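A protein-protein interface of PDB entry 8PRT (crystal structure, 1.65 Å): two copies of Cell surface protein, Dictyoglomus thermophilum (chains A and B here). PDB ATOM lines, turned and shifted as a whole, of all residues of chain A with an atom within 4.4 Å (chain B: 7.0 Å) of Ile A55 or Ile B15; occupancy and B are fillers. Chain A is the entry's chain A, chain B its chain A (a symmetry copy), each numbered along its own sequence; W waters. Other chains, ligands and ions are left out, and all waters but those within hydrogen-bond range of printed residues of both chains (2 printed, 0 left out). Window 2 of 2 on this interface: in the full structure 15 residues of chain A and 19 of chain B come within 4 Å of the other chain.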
ATOM      1  N   ALA A  14      -6.339  17.510  37.393  1.00  0.00           N
ATOM      2  CA  ALA A  14      -5.458  16.478  36.867  1.00  0.00           C
ATOM      3  C   ALA A  14      -4.585  15.948  37.986  1.00  0.00           C
ATOM      4  O   ALA A  14      -4.223  16.687  38.906  1.00  0.00           O
ATOM      5  CB  ALA A  14      -4.581  17.022  35.748  1.00  0.00           C
ATOM      6  N   ILE A  15      -4.223  14.662  37.895  1.00  0.00           N
ATOM      7  CA  ILE A  15      -3.456  14.022  38.959  1.00  0.00           C
ATOM      8  C   ILE A  15      -2.114  13.608  38.412  1.00  0.00           C
ATOM      9  O   ILE A  15      -2.049  12.844  37.440  1.00  0.00           O
ATOM     10  CB  ILE A  15      -4.195  12.811  39.552  1.00  0.00           C
ATOM     11  CG1 ILE A  15      -5.620  13.225  39.948  1.00  0.00           C
ATOM     12  CG2 ILE A  15      -3.420  12.271  40.735  1.00  0.00           C
ATOM     13  CD1 ILE A  15      -6.439  12.153  40.541  1.00  0.00           C
ATOM     14  N   GLY A  16      -1.045  14.094  39.052  1.00  0.00           N
ATOM     15  CA  GLY A  16       0.298  13.742  38.659  1.00  0.00           C
ATOM     16  C   GLY A  16       0.699  12.379  39.131  1.00  0.00           C
ATOM     17  O   GLY A  16       0.020  11.709  39.900  1.00  0.00           O
ATOM     18  N   GLN A  17       1.898  12.011  38.689  1.00  0.00           N
ATOM     19  CA  GLN A  17       2.479  10.699  38.869  1.00  0.00           C
ATOM     20  C   GLN A  17       2.775  10.416  40.333  1.00  0.00           C
ATOM     21  O   GLN A  17       2.777   9.247  40.750  1.00  0.00           O
ATOM     22  CB  GLN A  17       3.718  10.684  37.965  1.00  0.00           C
ATOM     23  CG  GLN A  17       3.384  11.248  36.521  1.00  0.00           C
ATOM     24  CD  GLN A  17       3.812  12.726  36.172  1.00  0.00           C
ATOM     25  OE1 GLN A  17       3.676  13.685  36.955  1.00  0.00           O
ATOM     26  NE2 GLN A  17       4.281  12.884  34.937  1.00  0.00           N
ATOM     27  N   TYR A  22      -3.662  19.047  40.347  1.00  0.00           N
ATOM     28  CA  TYR A  22      -3.561  20.344  39.702  1.00  0.00           C
ATOM     29  C   TYR A  22      -4.935  20.779  39.230  1.00  0.00           C
ATOM     30  O   TYR A  22      -5.668  19.991  38.645  1.00  0.00           O
ATOM     31  CB  TYR A  22      -2.619  20.297  38.506  1.00  0.00           C
ATOM     32  CG  TYR A  22      -1.238  19.719  38.805  1.00  0.00           C
ATOM     33  CD1 TYR A  22      -0.206  20.533  39.253  1.00  0.00           C
ATOM     34  CD2 TYR A  22      -0.977  18.369  38.635  1.00  0.00           C
ATOM     35  CE1 TYR A  22       1.065  20.004  39.517  1.00  0.00           C
ATOM     36  CE2 TYR A  22       0.267  17.849  38.891  1.00  0.00           C
ATOM     37  CZ  TYR A  22       1.280  18.662  39.322  1.00  0.00           C
ATOM     38  OH  TYR A  22       2.534  18.130  39.569  1.00  0.00           O
ATOM     39  N   ALA A  54      -3.453  19.440  31.714  1.00  0.00           N
ATOM     40  CA  ALA A  54      -2.926  18.165  31.240  1.00  0.00           C
ATOM     41  C   ALA A  54      -1.467  18.062  31.640  1.00  0.00           C
ATOM     42  O   ALA A  54      -0.767  19.066  31.746  1.00  0.00           O
ATOM     43  CB  ALA A  54      -3.038  18.030  29.726  1.00  0.00           C
ATOM     44  N   ILE A  55      -0.990  16.835  31.830  1.00  0.00           N
ATOM     45  CA  ILE A  55       0.369  16.607  32.317  1.00  0.00           C
ATOM     46  C   ILE A  55       1.146  15.867  31.245  1.00  0.00           C
ATOM     47  O   ILE A  55       0.729  14.784  30.810  1.00  0.00           O
ATOM     48  CB  ILE A  55       0.372  15.811  33.629  1.00  0.00           C
ATOM     49  CG1 ILE A  55      -0.521  16.500  34.657  1.00  0.00           C
ATOM     50  CG2 ILE A  55       1.782  15.694  34.161  1.00  0.00           C
ATOM     51  CD1 ILE A  55      -0.726  15.714  35.913  1.00  0.00           C
ATOM     52  N   GLY A  56       2.285  16.441  30.836  1.00  0.00           N
ATOM     53  CA  GLY A  56       3.152  15.813  29.855  1.00  0.00           C
ATOM     54  C   GLY A  56       3.999  14.699  30.451  1.00  0.00           C
ATOM     55  O   GLY A  56       4.031  14.473  31.657  1.00  0.00           O
ATOM     56  N   GLN A  57       4.726  14.005  29.572  1.00  0.00           N
ATOM     57  CA  GLN A  57       5.507  12.850  30.024  1.00  0.00           C
ATOM     58  C   GLN A  57       6.635  13.251  30.962  1.00  0.00           C
ATOM     59  O   GLN A  57       7.040  12.442  31.802  1.00  0.00           O
ATOM     60  CB  GLN A  57       6.074  12.079  28.830  1.00  0.00           C
ATOM     61  CG  GLN A  57       5.029  11.677  27.814  1.00  0.00           C
ATOM     62  CD  GLN A  57       5.523  10.728  26.729  1.00  0.00           C
ATOM     63  OE1 GLN A  57       4.803  10.471  25.767  1.00  0.00           O
ATOM     64  NE2 GLN A  57       6.736  10.201  26.883  1.00  0.00           N
ATOM     65  N   GLY A  59       6.290  15.682  33.106  1.00  0.00           N
ATOM     66  CA  GLY A  59       5.627  16.295  34.236  1.00  0.00           C
ATOM     67  C   GLY A  59       5.171  17.710  34.006  1.00  0.00           C
ATOM     68  O   GLY A  59       4.513  18.288  34.891  1.00  0.00           O
ATOM     69  N   THR A  60       5.523  18.306  32.875  1.00  0.00           N
ATOM     70  CA  THR A  60       5.048  19.659  32.595  1.00  0.00           C
ATOM     71  C   THR A  60       3.533  19.690  32.690  1.00  0.00           C
ATOM     72  O   THR A  60       2.842  18.772  32.235  1.00  0.00           O
ATOM     73  CB  THR A  60       5.482  20.112  31.198  1.00  0.00           C
ATOM     74  OG1 THR A  60       6.892  19.987  31.044  1.00  0.00           O
ATOM     75  CG2 THR A  60       5.122  21.566  30.951  1.00  0.00           C
ATOM     76  N   TYR A  62       0.198  21.691  31.549  1.00  0.00           N
ATOM     77  CA  TYR A  62      -0.307  22.602  30.528  1.00  0.00           C
ATOM     78  C   TYR A  62      -1.746  22.974  30.843  1.00  0.00           C
ATOM     79  O   TYR A  62      -2.557  22.102  31.181  1.00  0.00           O
ATOM     80  CB  TYR A  62      -0.272  21.962  29.140  1.00  0.00           C
ATOM     81  CG  TYR A  62       1.078  21.411  28.747  1.00  0.00           C
ATOM     82  CD1 TYR A  62       2.036  22.218  28.143  1.00  0.00           C
ATOM     83  CD2 TYR A  62       1.378  20.075  28.958  1.00  0.00           C
ATOM     84  CE1 TYR A  62       3.289  21.692  27.777  1.00  0.00           C
ATOM     85  CE2 TYR A  62       2.597  19.561  28.599  1.00  0.00           C
ATOM     86  CZ  TYR A  62       3.540  20.369  28.010  1.00  0.00           C
ATOM     87  OH  TYR A  62       4.756  19.846  27.640  1.00  0.00           O
ATOM     88  N   PRO B  13      -6.194  21.128  27.212  1.00  0.00           N
ATOM     89  CA  PRO B  13      -5.219  20.556  26.279  1.00  0.00           C
ATOM     90  C   PRO B  13      -5.202  19.032  26.292  1.00  0.00           C
ATOM     91  O   PRO B  13      -5.421  18.381  27.319  1.00  0.00           O
ATOM     92  CB  PRO B  13      -3.883  21.133  26.761  1.00  0.00           C
ATOM     93  CG  PRO B  13      -4.131  21.612  28.168  1.00  0.00           C
ATOM     94  CD  PRO B  13      -5.559  21.977  28.243  1.00  0.00           C
ATOM     95  N   ALA B  14      -4.901  18.473  25.127  1.00  0.00           N
ATOM     96  CA  ALA B  14      -4.573  17.062  24.985  1.00  0.00           C
ATOM     97  C   ALA B  14      -3.124  16.924  24.566  1.00  0.00           C
ATOM     98  O   ALA B  14      -2.592  17.776  23.850  1.00  0.00           O
ATOM     99  CB  ALA B  14      -5.471  16.392  23.955  1.00  0.00           C
ATOM    100  N   ILE B  15      -2.487  15.828  24.995  1.00  0.00           N
ATOM    101  CA  ILE B  15      -1.066  15.633  24.726  1.00  0.00           C
ATOM    102  C   ILE B  15      -0.897  14.416  23.854  1.00  0.00           C
ATOM    103  O   ILE B  15      -1.323  13.317  24.233  1.00  0.00           O
ATOM    104  CB  ILE B  15      -0.249  15.488  26.021  1.00  0.00           C
ATOM    105  CG1 ILE B  15      -0.569  16.660  26.961  1.00  0.00           C
ATOM    106  CG2 ILE B  15       1.226  15.426  25.688  1.00  0.00           C
ATOM    107  CD1 ILE B  15       0.157  16.648  28.243  1.00  0.00           C
ATOM    108  N   GLY B  16      -0.252  14.608  22.698  1.00  0.00           N
ATOM    109  CA  GLY B  16       0.015  13.518  21.790  1.00  0.00           C
ATOM    110  C   GLY B  16       1.167  12.668  22.231  1.00  0.00           C
ATOM    111  O   GLY B  16       1.896  12.964  23.171  1.00  0.00           O
ATOM    112  N   GLN B  17       1.355  11.608  21.452  1.00  0.00           N
ATOM    113  CA  GLN B  17       2.299  10.545  21.716  1.00  0.00           C
ATOM    114  C   GLN B  17       3.734  11.039  21.633  1.00  0.00           C
ATOM    115  O   GLN B  17       4.622  10.478  22.293  1.00  0.00           O
ATOM    116  CB  GLN B  17       1.955   9.446  20.703  1.00  0.00           C
ATOM    117  CG  GLN B  17       0.393   9.171  20.659  1.00  0.00           C
ATOM    118  CD  GLN B  17      -0.445   9.781  19.470  1.00  0.00           C
ATOM    119  OE1 GLN B  17      -0.287  10.939  19.038  1.00  0.00           O
ATOM    120  NE2 GLN B  17      -1.389   8.972  18.993  1.00  0.00           N
ATOM    121  N   ASP B  18       3.960  12.127  20.893  1.00  0.00           N
ATOM    122  CA  ASP B  18       5.250  12.766  20.717  1.00  0.00           C
ATOM    123  C   ASP B  18       5.365  14.049  21.536  1.00  0.00           C
ATOM    124  O   ASP B  18       6.334  14.789  21.383  1.00  0.00           O
ATOM    125  CB  ASP B  18       5.514  13.060  19.243  1.00  0.00           C
ATOM    126  CG  ASP B  18       4.599  14.126  18.675  1.00  0.00           C
ATOM    127  OD1 ASP B  18       3.601  14.527  19.330  1.00  0.00           O
ATOM    128  OD2 ASP B  18       4.884  14.569  17.551  1.00  0.00           O
ATOM    129  N   GLY B  19       4.413  14.314  22.423  1.00  0.00           N
ATOM    130  CA  GLY B  19       4.474  15.488  23.269  1.00  0.00           C
ATOM    131  C   GLY B  19       3.764  16.704  22.725  1.00  0.00           C
ATOM    132  O   GLY B  19       3.655  17.705  23.443  1.00  0.00           O
ATOM    133  N   THR B  20       3.286  16.661  21.485  1.00  0.00           N
ATOM    134  CA  THR B  20       2.542  17.798  20.947  1.00  0.00           C
ATOM    135  C   THR B  20       1.340  18.094  21.832  1.00  0.00           C
ATOM    136  O   THR B  20       0.652  17.179  22.292  1.00  0.00           O
ATOM    137  CB  THR B  20       2.074  17.503  19.512  1.00  0.00           C
ATOM    138  OG1 THR B  20       3.209  17.143  18.694  1.00  0.00           O
ATOM    139  CG2 THR B  20       1.397  18.710  18.889  1.00  0.00           C
ATOM    140  N   ILE B  21       1.081  19.384  22.067  1.00  0.00           N
ATOM    141  CA  ILE B  21      -0.040  19.845  22.892  1.00  0.00           C
ATOM    142  C   ILE B  21      -1.088  20.441  21.970  1.00  0.00           C
ATOM    143  O   ILE B  21      -0.787  21.348  21.201  1.00  0.00           O
ATOM    144  CB  ILE B  21       0.414  20.861  23.948  1.00  0.00           C
ATOM    145  CG1 ILE B  21       1.597  20.310  24.749  1.00  0.00           C
ATOM    146  CG2 ILE B  21      -0.710  21.185  24.919  1.00  0.00           C
ATOM    147  CD1 ILE B  21       2.932  20.887  24.358  1.00  0.00           C
ATOM    148  N   TYR B  22      -2.320  19.933  22.051  1.00  0.00           N
ATOM    149  CA  TYR B  22      -3.423  20.405  21.232  1.00  0.00           C
ATOM    150  C   TYR B  22      -4.454  21.077  22.119  1.00  0.00           C
ATOM    151  O   TYR B  22      -4.805  20.554  23.169  1.00  0.00           O
ATOM    152  CB  TYR B  22      -4.089  19.258  20.483  1.00  0.00           C
ATOM    153  CG  TYR B  22      -3.132  18.387  19.672  1.00  0.00           C
ATOM    154  CD1 TYR B  22      -2.811  18.711  18.361  1.00  0.00           C
ATOM    155  CD2 TYR B  22      -2.562  17.250  20.221  1.00  0.00           C
ATOM    156  CE1 TYR B  22      -1.941  17.906  17.612  1.00  0.00           C
ATOM    157  CE2 TYR B  22      -1.712  16.459  19.490  1.00  0.00           C
ATOM    158  CZ  TYR B  22      -1.410  16.782  18.195  1.00  0.00           C
ATOM    159  OH  TYR B  22      -0.559  15.972  17.463  1.00  0.00           O
ATOM    160  N   PRO B  53      -9.849  18.657  22.880  1.00  0.00           N
ATOM    161  CA  PRO B  53      -9.536  17.635  21.872  1.00  0.00           C
ATOM    162  C   PRO B  53      -9.266  16.257  22.462  1.00  0.00           C
ATOM    163  O   PRO B  53      -8.815  16.106  23.602  1.00  0.00           O
ATOM    164  CB  PRO B  53      -8.289  18.196  21.176  1.00  0.00           C
ATOM    165  CG  PRO B  53      -7.726  19.200  22.121  1.00  0.00           C
ATOM    166  CD  PRO B  53      -8.860  19.753  22.891  1.00  0.00           C
ATOM    167  N   ILE B  55      -7.473  12.376  21.101  1.00  0.00           N
ATOM    168  CA  ILE B  55      -6.532  11.859  20.109  1.00  0.00           C
ATOM    169  C   ILE B  55      -6.824  10.388  19.888  1.00  0.00           C
ATOM    170  O   ILE B  55      -6.814   9.600  20.845  1.00  0.00           O
ATOM    171  CB  ILE B  55      -5.077  12.056  20.558  1.00  0.00           C
ATOM    172  CG1 ILE B  55      -4.834  13.522  20.904  1.00  0.00           C
ATOM    173  CG2 ILE B  55      -4.133  11.617  19.462  1.00  0.00           C
ATOM    174  CD1 ILE B  55      -3.496  13.791  21.518  1.00  0.00           C
HETATM  175  O   HOH W   1       3.108  12.447  25.695  1.00  0.00           O
HETATM  176  O   HOH W   2       4.398  17.387  26.013  1.00  0.00           O
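Ile A55 touches one residue of chain B.
Of chain A, only Ala A54, Ile A55, Gly A56 and Tyr A62 come within 4 Å of Ile B15.
Of the printed residues of chain B, Tyr A62 touches Pro B13 (3.4 Å), Ile B15 (3.7 Å) and Ile B21 (3.5 Å).
Printed residues of chain B within 4 Å of Ala A54: Pro B13 and Ile B15.
Gln A17 touches none of the printed residues of chain B.
The nearest residue of chain B that does not touch Ile A55 is Pro B13 (6.5 Å).
The nearest printed residue of chain B that does not touch Gly A56 is Gly B19 (6.7 Å).
Water W1 bridges OE1 of Gln A57 and O of Gly B16.
Water W2 lies within hydrogen-bond range of O of Gly B19 (2.7 Å) and OH of Tyr A62 (3.0 Å).
The backbone carbonyl oxygen (O) of Gln B17 lies close to the side-chain amide oxygen (OE1) of Gln A57 (3.5 Å).
Ile A55 touches Ile B15, but with the chains exchanged Ile A15 does not touch Ile B55 (16.0 Å).
6 positions are printed for both chains.
Of the 8 pairs that touch across the chains among the printed residues, none has its exchanged pair printed and touching as well.
Hydrophobic or aromatic side chains of chain B that line the printed part of chain A: Pro B13, Ile B15 and Ile B21.
Of the 12 printed residues of chain A, 5 touch a printed residue of chain B.
Hydrophobic or aromatic side chains of chain A within 4 Å of the printed part of chain B: Ala A54 and Tyr A62.
Among the printed residues, no Asp or Glu carboxylate lies within 4 Å of a Lys or Arg side-chain nitrogen of the other chain.
Ala A54 touches Pro B13 (CB to O, 3.4 Å).
Ala A54 touches Ile B15 (CB to CD1, 3.8 Å).
Ile B15 touches Ile A55.
N of Gly A56 touches CD1 of Ile B15 (3.4 Å).
Tyr A62 touches Pro B13 (O to CG, 3.4 Å).
Tyr A62 touches Ile B15 (CD2 to CD1, 3.7 Å).
CD1 of Ile B21 touches CE1 of Tyr A62, 3.5 Å away.
N of Tyr A62 sits at hydrogen-bond distance from O of Ala A54, at 2.8 Å.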
